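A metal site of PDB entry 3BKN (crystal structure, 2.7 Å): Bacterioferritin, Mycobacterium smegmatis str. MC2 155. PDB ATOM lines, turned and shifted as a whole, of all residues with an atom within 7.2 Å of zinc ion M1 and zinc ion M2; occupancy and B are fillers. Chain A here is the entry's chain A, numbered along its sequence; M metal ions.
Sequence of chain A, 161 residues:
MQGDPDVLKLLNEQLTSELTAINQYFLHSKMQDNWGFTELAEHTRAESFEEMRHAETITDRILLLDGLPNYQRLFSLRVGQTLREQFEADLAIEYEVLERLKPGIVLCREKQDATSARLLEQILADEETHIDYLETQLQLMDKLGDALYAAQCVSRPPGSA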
ATOM      1  N   GLN A  14      -5.913 -28.723 -10.279  1.00  0.00           N
ATOM      2  CA  GLN A  14      -5.838 -27.280 -10.388  1.00  0.00           C
ATOM      3  C   GLN A  14      -6.096 -26.801 -11.825  1.00  0.00           C
ATOM      4  O   GLN A  14      -6.794 -25.791 -12.036  1.00  0.00           O
ATOM      5  CB  GLN A  14      -4.500 -26.771  -9.958  1.00  0.00           C
ATOM      6  CG  GLN A  14      -4.452 -25.253  -9.839  1.00  0.00           C
ATOM      7  CD  GLN A  14      -5.541 -24.700  -8.912  1.00  0.00           C
ATOM      8  OE1 GLN A  14      -6.111 -25.450  -8.096  1.00  0.00           O
ATOM      9  NE2 GLN A  14      -5.842 -23.403  -9.047  1.00  0.00           N
ATOM     10  N   SER A  17      -9.681 -26.621 -12.464  1.00  0.00           N
ATOM     11  CA  SER A  17     -10.196 -25.361 -11.863  1.00  0.00           C
ATOM     12  C   SER A  17      -9.931 -24.120 -12.726  1.00  0.00           C
ATOM     13  O   SER A  17     -10.850 -23.311 -12.920  1.00  0.00           O
ATOM     14  CB  SER A  17      -9.663 -25.095 -10.458  1.00  0.00           C
ATOM     15  OG  SER A  17     -10.569 -25.532  -9.480  1.00  0.00           O
ATOM     16  N   GLU A  18      -8.708 -23.960 -13.240  1.00  0.00           N
ATOM     17  CA  GLU A  18      -8.455 -22.851 -14.145  1.00  0.00           C
ATOM     18  C   GLU A  18      -9.294 -22.930 -15.435  1.00  0.00           C
ATOM     19  O   GLU A  18      -9.781 -21.898 -15.930  1.00  0.00           O
ATOM     20  CB  GLU A  18      -6.991 -22.687 -14.548  1.00  0.00           C
ATOM     21  CG  GLU A  18      -6.016 -22.848 -13.502  1.00  0.00           C
ATOM     22  CD  GLU A  18      -5.977 -21.721 -12.503  1.00  0.00           C
ATOM     23  OE1 GLU A  18      -6.498 -20.624 -12.778  1.00  0.00           O
ATOM     24  OE2 GLU A  18      -5.361 -21.929 -11.458  1.00  0.00           O
ATOM     25  N   ALA A  21     -12.587 -21.739 -14.419  1.00  0.00           N
ATOM     26  CA  ALA A  21     -12.569 -20.283 -14.199  1.00  0.00           C
ATOM     27  C   ALA A  21     -12.479 -19.487 -15.526  1.00  0.00           C
ATOM     28  O   ALA A  21     -13.153 -18.495 -15.680  1.00  0.00           O
ATOM     29  CB  ALA A  21     -11.480 -19.869 -13.215  1.00  0.00           C
ATOM     30  N   TYR A  25     -15.524 -16.746 -15.850  1.00  0.00           N
ATOM     31  CA  TYR A  25     -15.191 -15.324 -16.002  1.00  0.00           C
ATOM     32  C   TYR A  25     -15.481 -14.802 -17.398  1.00  0.00           C
ATOM     33  O   TYR A  25     -16.132 -13.768 -17.567  1.00  0.00           O
ATOM     34  CB  TYR A  25     -13.736 -15.096 -15.712  1.00  0.00           C
ATOM     35  CG  TYR A  25     -13.367 -15.072 -14.261  1.00  0.00           C
ATOM     36  CD1 TYR A  25     -13.834 -14.032 -13.418  1.00  0.00           C
ATOM     37  CD2 TYR A  25     -12.511 -16.007 -13.730  1.00  0.00           C
ATOM     38  CE1 TYR A  25     -13.496 -13.983 -12.095  1.00  0.00           C
ATOM     39  CE2 TYR A  25     -12.145 -15.969 -12.386  1.00  0.00           C
ATOM     40  CZ  TYR A  25     -12.626 -14.946 -11.583  1.00  0.00           C
ATOM     41  OH  TYR A  25     -12.266 -14.851 -10.221  1.00  0.00           O
ATOM     42  N   GLU A  47      -9.727 -10.679 -15.620  1.00  0.00           N
ATOM     43  CA  GLU A  47      -9.652 -11.834 -14.734  1.00  0.00           C
ATOM     44  C   GLU A  47      -9.632 -13.159 -15.508  1.00  0.00           C
ATOM     45  O   GLU A  47      -8.870 -14.086 -15.188  1.00  0.00           O
ATOM     46  CB  GLU A  47     -10.769 -11.776 -13.686  1.00  0.00           C
ATOM     47  CG  GLU A  47     -10.768 -10.466 -12.868  1.00  0.00           C
ATOM     48  CD  GLU A  47      -9.651 -10.401 -11.831  1.00  0.00           C
ATOM     49  OE1 GLU A  47      -8.684 -11.181 -11.952  1.00  0.00           O
ATOM     50  OE2 GLU A  47      -9.748  -9.582 -10.885  1.00  0.00           O
ATOM     51  N   GLU A  50      -6.144 -13.790 -16.922  1.00  0.00           N
ATOM     52  CA  GLU A  50      -5.275 -14.244 -15.862  1.00  0.00           C
ATOM     53  C   GLU A  50      -5.477 -15.714 -15.630  1.00  0.00           C
ATOM     54  O   GLU A  50      -4.513 -16.408 -15.390  1.00  0.00           O
ATOM     55  CB  GLU A  50      -5.484 -13.456 -14.566  1.00  0.00           C
ATOM     56  CG  GLU A  50      -4.155 -12.796 -14.084  1.00  0.00           C
ATOM     57  CD  GLU A  50      -4.162 -12.333 -12.635  1.00  0.00           C
ATOM     58  OE1 GLU A  50      -4.663 -11.199 -12.365  1.00  0.00           O
ATOM     59  OE2 GLU A  50      -3.641 -13.093 -11.779  1.00  0.00           O
ATOM     60  N   GLU A  51      -6.708 -16.220 -15.729  1.00  0.00           N
ATOM     61  CA  GLU A  51      -6.934 -17.636 -15.627  1.00  0.00           C
ATOM     62  C   GLU A  51      -6.350 -18.371 -16.788  1.00  0.00           C
ATOM     63  O   GLU A  51      -5.780 -19.442 -16.606  1.00  0.00           O
ATOM     64  CB  GLU A  51      -8.386 -17.998 -15.476  1.00  0.00           C
ATOM     65  CG  GLU A  51      -9.005 -17.409 -14.288  1.00  0.00           C
ATOM     66  CD  GLU A  51      -8.270 -17.667 -12.974  1.00  0.00           C
ATOM     67  OE1 GLU A  51      -7.287 -18.441 -12.940  1.00  0.00           O
ATOM     68  OE2 GLU A  51      -8.651 -17.053 -11.954  1.00  0.00           O
ATOM     69  N   MET A  52      -6.494 -17.829 -17.999  1.00  0.00           N
ATOM     70  CA  MET A  52      -5.863 -18.438 -19.164  1.00  0.00           C
ATOM     71  C   MET A  52      -4.353 -18.604 -18.952  1.00  0.00           C
ATOM     72  O   MET A  52      -3.791 -19.665 -19.266  1.00  0.00           O
ATOM     73  CB  MET A  52      -6.134 -17.635 -20.417  1.00  0.00           C
ATOM     74  CG  MET A  52      -7.547 -17.703 -20.895  1.00  0.00           C
ATOM     75  SD  MET A  52      -7.881 -16.578 -22.284  1.00  0.00           S
ATOM     76  CE  MET A  52      -9.543 -16.033 -21.828  1.00  0.00           C
ATOM     77  N   ARG A  53      -3.697 -17.579 -18.405  1.00  0.00           N
ATOM     78  CA  ARG A  53      -2.279 -17.688 -18.091  1.00  0.00           C
ATOM     79  C   ARG A  53      -1.989 -18.783 -17.036  1.00  0.00           C
ATOM     80  O   ARG A  53      -1.027 -19.560 -17.216  1.00  0.00           O
ATOM     81  CB  ARG A  53      -1.687 -16.343 -17.725  1.00  0.00           C
ATOM     82  CG  ARG A  53      -1.662 -15.386 -18.904  1.00  0.00           C
ATOM     83  CD  ARG A  53      -1.126 -13.978 -18.554  1.00  0.00           C
ATOM     84  NE  ARG A  53      -2.161 -13.208 -17.883  1.00  0.00           N
ATOM     85  CZ  ARG A  53      -1.977 -12.032 -17.304  1.00  0.00           C
ATOM     86  NH1 ARG A  53      -0.788 -11.456 -17.312  1.00  0.00           N
ATOM     87  NH2 ARG A  53      -2.994 -11.433 -16.708  1.00  0.00           N
ATOM     88  N   HIS A  54      -2.809 -18.883 -15.995  1.00  0.00           N
ATOM     89  CA  HIS A  54      -2.669 -19.939 -15.019  1.00  0.00           C
ATOM     90  C   HIS A  54      -2.732 -21.349 -15.658  1.00  0.00           C
ATOM     91  O   HIS A  54      -1.862 -22.209 -15.394  1.00  0.00           O
ATOM     92  CB  HIS A  54      -3.757 -19.806 -13.978  1.00  0.00           C
ATOM     93  CG  HIS A  54      -3.551 -18.662 -13.068  1.00  0.00           C
ATOM     94  ND1 HIS A  54      -4.491 -18.283 -12.123  1.00  0.00           N
ATOM     95  CD2 HIS A  54      -2.530 -17.775 -12.970  1.00  0.00           C
ATOM     96  CE1 HIS A  54      -4.027 -17.244 -11.451  1.00  0.00           C
ATOM     97  NE2 HIS A  54      -2.848 -16.916 -11.961  1.00  0.00           N
ATOM     98  N   ALA A  55      -3.756 -21.569 -16.473  1.00  0.00           N
ATOM     99  CA  ALA A  55      -3.883 -22.805 -17.215  1.00  0.00           C
ATOM    100  C   ALA A  55      -2.599 -23.090 -17.994  1.00  0.00           C
ATOM    101  O   ALA A  55      -2.103 -24.209 -17.982  1.00  0.00           O
ATOM    102  CB  ALA A  55      -5.108 -22.781 -18.146  1.00  0.00           C
ATOM    103  N   ILE A  58       0.451 -24.081 -15.614  1.00  0.00           N
ATOM    104  CA  ILE A  58       0.233 -25.430 -15.128  1.00  0.00           C
ATOM    105  C   ILE A  58       0.465 -26.480 -16.233  1.00  0.00           C
ATOM    106  O   ILE A  58       1.134 -27.475 -15.989  1.00  0.00           O
ATOM    107  CB  ILE A  58      -1.166 -25.582 -14.450  1.00  0.00           C
ATOM    108  CG1 ILE A  58      -1.225 -24.838 -13.106  1.00  0.00           C
ATOM    109  CG2 ILE A  58      -1.527 -27.070 -14.206  1.00  0.00           C
ATOM    110  CD1 ILE A  58      -2.678 -24.395 -12.698  1.00  0.00           C
ATOM    111  N   ASP A  90     -18.064 -16.391  -8.815  1.00  0.00           N
ATOM    112  CA  ASP A  90     -16.606 -16.369  -9.011  1.00  0.00           C
ATOM    113  C   ASP A  90     -15.861 -16.491  -7.668  1.00  0.00           C
ATOM    114  O   ASP A  90     -14.826 -17.142  -7.557  1.00  0.00           O
ATOM    115  CB  ASP A  90     -16.185 -15.137  -9.818  1.00  0.00           C
ATOM    116  CG  ASP A  90     -16.750 -15.152 -11.265  1.00  0.00           C
ATOM    117  OD1 ASP A  90     -16.841 -16.269 -11.854  1.00  0.00           O
ATOM    118  OD2 ASP A  90     -17.117 -14.052 -11.802  1.00  0.00           O
ATOM    119  N   ILE A  93     -15.618 -20.298  -6.755  1.00  0.00           N
ATOM    120  CA  ILE A  93     -14.488 -21.061  -7.256  1.00  0.00           C
ATOM    121  C   ILE A  93     -13.095 -20.629  -6.770  1.00  0.00           C
ATOM    122  O   ILE A  93     -12.180 -21.464  -6.709  1.00  0.00           O
ATOM    123  CB  ILE A  93     -14.446 -21.313  -8.772  1.00  0.00           C
ATOM    124  CG1 ILE A  93     -14.713 -20.083  -9.561  1.00  0.00           C
ATOM    125  CG2 ILE A  93     -15.387 -22.493  -9.178  1.00  0.00           C
ATOM    126  CD1 ILE A  93     -14.754 -20.454 -11.027  1.00  0.00           C
ATOM    127  N   GLU A  94     -12.922 -19.351  -6.451  1.00  0.00           N
ATOM    128  CA  GLU A  94     -11.643 -18.934  -5.901  1.00  0.00           C
ATOM    129  C   GLU A  94     -11.431 -19.593  -4.558  1.00  0.00           C
ATOM    130  O   GLU A  94     -10.321 -20.045  -4.279  1.00  0.00           O
ATOM    131  CB  GLU A  94     -11.517 -17.421  -5.843  1.00  0.00           C
ATOM    132  CG  GLU A  94     -11.563 -16.756  -7.203  1.00  0.00           C
ATOM    133  CD  GLU A  94     -10.339 -17.042  -8.060  1.00  0.00           C
ATOM    134  OE1 GLU A  94      -9.418 -17.791  -7.647  1.00  0.00           O
ATOM    135  OE2 GLU A  94     -10.291 -16.513  -9.184  1.00  0.00           O
ATOM    136  N   VAL A  97     -10.251 -23.050  -4.923  1.00  0.00           N
ATOM    137  CA  VAL A  97      -8.834 -23.068  -5.220  1.00  0.00           C
ATOM    138  C   VAL A  97      -7.992 -22.993  -3.938  1.00  0.00           C
ATOM    139  O   VAL A  97      -7.085 -23.802  -3.756  1.00  0.00           O
ATOM    140  CB  VAL A  97      -8.491 -22.037  -6.284  1.00  0.00           C
ATOM    141  CG1 VAL A  97      -6.985 -21.859  -6.385  1.00  0.00           C
ATOM    142  CG2 VAL A  97      -9.077 -22.498  -7.621  1.00  0.00           C
ATOM    143  N   ILE A 123       0.302 -19.039  -7.997  1.00  0.00           N
ATOM    144  CA  ILE A 123      -1.086 -19.076  -8.329  1.00  0.00           C
ATOM    145  C   ILE A 123      -1.955 -18.698  -7.113  1.00  0.00           C
ATOM    146  O   ILE A 123      -2.842 -17.834  -7.216  1.00  0.00           O
ATOM    147  CB  ILE A 123      -1.460 -20.395  -9.022  1.00  0.00           C
ATOM    148  CG1 ILE A 123      -1.021 -20.304 -10.499  1.00  0.00           C
ATOM    149  CG2 ILE A 123      -2.947 -20.679  -8.947  1.00  0.00           C
ATOM    150  CD1 ILE A 123      -0.795 -21.593 -11.094  1.00  0.00           C
ATOM    151  N   LEU A 124      -1.654 -19.288  -5.963  1.00  0.00           N
ATOM    152  CA  LEU A 124      -2.391 -19.008  -4.734  1.00  0.00           C
ATOM    153  C   LEU A 124      -2.432 -17.518  -4.440  1.00  0.00           C
ATOM    154  O   LEU A 124      -3.504 -16.955  -4.172  1.00  0.00           O
ATOM    155  CB  LEU A 124      -1.833 -19.782  -3.530  1.00  0.00           C
ATOM    156  CG  LEU A 124      -2.534 -19.686  -2.166  1.00  0.00           C
ATOM    157  CD1 LEU A 124      -4.046 -19.915  -2.243  1.00  0.00           C
ATOM    158  CD2 LEU A 124      -1.926 -20.619  -1.159  1.00  0.00           C
ATOM    159  N   ASP A 126      -2.075 -14.981  -6.557  1.00  0.00           N
ATOM    160  CA  ASP A 126      -2.981 -14.381  -7.523  1.00  0.00           C
ATOM    161  C   ASP A 126      -4.451 -14.663  -7.122  1.00  0.00           C
ATOM    162  O   ASP A 126      -5.255 -13.747  -7.055  1.00  0.00           O
ATOM    163  CB  ASP A 126      -2.698 -14.830  -8.971  1.00  0.00           C
ATOM    164  CG  ASP A 126      -1.278 -14.401  -9.493  1.00  0.00           C
ATOM    165  OD1 ASP A 126      -0.434 -13.784  -8.792  1.00  0.00           O
ATOM    166  OD2 ASP A 126      -0.975 -14.707 -10.658  1.00  0.00           O
ATOM    167  N   GLU A 127      -4.798 -15.888  -6.785  1.00  0.00           N
ATOM    168  CA  GLU A 127      -6.207 -16.118  -6.418  1.00  0.00           C
ATOM    169  C   GLU A 127      -6.628 -15.421  -5.142  1.00  0.00           C
ATOM    170  O   GLU A 127      -7.795 -15.079  -5.014  1.00  0.00           O
ATOM    171  CB  GLU A 127      -6.602 -17.606  -6.415  1.00  0.00           C
ATOM    172  CG  GLU A 127      -5.946 -18.445  -7.448  1.00  0.00           C
ATOM    173  CD  GLU A 127      -6.530 -18.289  -8.821  1.00  0.00           C
ATOM    174  OE1 GLU A 127      -6.904 -17.154  -9.175  1.00  0.00           O
ATOM    175  OE2 GLU A 127      -6.587 -19.291  -9.579  1.00  0.00           O
ATOM    176  N   GLU A 128      -5.724 -15.199  -4.206  1.00  0.00           N
ATOM    177  CA  GLU A 128      -6.086 -14.491  -2.968  1.00  0.00           C
ATOM    178  C   GLU A 128      -6.396 -13.050  -3.338  1.00  0.00           C
ATOM    179  O   GLU A 128      -7.313 -12.454  -2.800  1.00  0.00           O
ATOM    180  CB  GLU A 128      -4.997 -14.567  -1.906  1.00  0.00           C
ATOM    181  CG  GLU A 128      -4.840 -15.924  -1.257  1.00  0.00           C
ATOM    182  CD  GLU A 128      -3.851 -15.967  -0.061  1.00  0.00           C
ATOM    183  OE1 GLU A 128      -3.786 -14.977   0.714  1.00  0.00           O
ATOM    184  OE2 GLU A 128      -3.156 -16.994   0.147  1.00  0.00           O
ATOM    185  N   THR A 129      -5.690 -12.510  -4.300  1.00  0.00           N
ATOM    186  CA  THR A 129      -5.994 -11.177  -4.775  1.00  0.00           C
ATOM    187  C   THR A 129      -7.386 -11.070  -5.462  1.00  0.00           C
ATOM    188  O   THR A 129      -8.095 -10.081  -5.243  1.00  0.00           O
ATOM    189  CB  THR A 129      -4.817 -10.639  -5.615  1.00  0.00           C
ATOM    190  OG1 THR A 129      -3.736 -10.390  -4.713  1.00  0.00           O
ATOM    191  CG2 THR A 129      -5.159  -9.348  -6.357  1.00  0.00           C
ATOM    192  N   HIS A 130      -7.766 -12.084  -6.241  1.00  0.00           N
ATOM    193  CA  HIS A 130      -9.087 -12.124  -6.848  1.00  0.00           C
ATOM    194  C   HIS A 130     -10.108 -12.178  -5.732  1.00  0.00           C
ATOM    195  O   HIS A 130     -11.074 -11.437  -5.771  1.00  0.00           O
ATOM    196  CB  HIS A 130      -9.305 -13.315  -7.806  1.00  0.00           C
ATOM    197  CG  HIS A 130      -8.500 -13.255  -9.088  1.00  0.00           C
ATOM    198  ND1 HIS A 130      -8.473 -14.303  -9.987  1.00  0.00           N
ATOM    199  CD2 HIS A 130      -7.669 -12.302  -9.591  1.00  0.00           C
ATOM    200  CE1 HIS A 130      -7.679 -14.000 -11.003  1.00  0.00           C
ATOM    201  NE2 HIS A 130      -7.168 -12.796 -10.788  1.00  0.00           N
ATOM    202  N   ILE A 131      -9.883 -13.003  -4.722  1.00  0.00           N
ATOM    203  CA  ILE A 131     -10.809 -13.084  -3.587  1.00  0.00           C
ATOM    204  C   ILE A 131     -10.973 -11.753  -2.910  1.00  0.00           C
ATOM    205  O   ILE A 131     -12.069 -11.375  -2.584  1.00  0.00           O
ATOM    206  CB  ILE A 131     -10.380 -14.166  -2.534  1.00  0.00           C
ATOM    207  CG1 ILE A 131     -10.547 -15.570  -3.129  1.00  0.00           C
ATOM    208  CG2 ILE A 131     -11.184 -14.033  -1.229  1.00  0.00           C
ATOM    209  CD1 ILE A 131      -9.716 -16.615  -2.453  1.00  0.00           C
ATOM    210  N   LEU A 134     -13.148  -9.479  -5.088  1.00  0.00           N
ATOM    211  CA  LEU A 134     -14.519  -9.969  -5.109  1.00  0.00           C
ATOM    212  C   LEU A 134     -15.239  -9.675  -3.828  1.00  0.00           C
ATOM    213  O   LEU A 134     -16.382  -9.198  -3.846  1.00  0.00           O
ATOM    214  CB  LEU A 134     -14.552 -11.462  -5.337  1.00  0.00           C
ATOM    215  CG  LEU A 134     -14.098 -11.949  -6.725  1.00  0.00           C
ATOM    216  CD1 LEU A 134     -13.862 -13.436  -6.705  1.00  0.00           C
ATOM    217  CD2 LEU A 134     -15.124 -11.563  -7.772  1.00  0.00           C
HETATM  218 ZN    ZN M   1      -6.193 -19.178 -11.496  1.00  0.00          ZN
HETATM  219 ZN    ZN M   2      -8.463 -16.442 -10.024  1.00  0.00          ZN
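Four residues have an atom within 4 Å of zinc ion M1: Glu 18, Glu 51, His 54 and Glu 127. The nearest printed residue that does not touch zinc ion M1 is Ile 123 (4.4 Å).
OE1 of Glu 18 is bound to zinc ion M1 (2.0 Å). OE1 of Glu 51 is bound to zinc ion M1, at 2.0 Å. Zinc ion M1 is bound by OE2 of Glu 127 (2.0 Å). A ring nitrogen (ND1) of His 54 binds zinc ion M1 (2.0 Å). Zinc ion M1 has four donor atoms within binding distance.
Zinc ion M2 is bound by the side-chain carboxylate of Glu 127 (1.9 Å), the side-chain carboxylate of Glu 94 (2.0 Å), the side-chain carboxylate of Glu 51 (2.0 Å) and a ring nitrogen (ND1) of His 130 (2.1 Å). Zinc ion M2 has four donor atoms within binding distance.
The side-chain carboxylate (OE2) of Glu 18 lies within hydrogen-bond range of the side-chain amide nitrogen (NE2) of Gln 14, at 2.9 Å. NE2 of His 130 is in hydrogen-bond range of OE1 of Glu 47. OH of Tyr 25 sits close to OE2 of Glu 94 (2.8 Å). A ring nitrogen (NE2) of His 54 sits at hydrogen-bond distance from the side-chain carboxylate of Asp 126 (3.2 Å). The side-chain carboxylate (OE1) of Glu 50 sits at hydrogen-bond distance from a ring nitrogen (NE2) of His 130 (3.4 Å).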
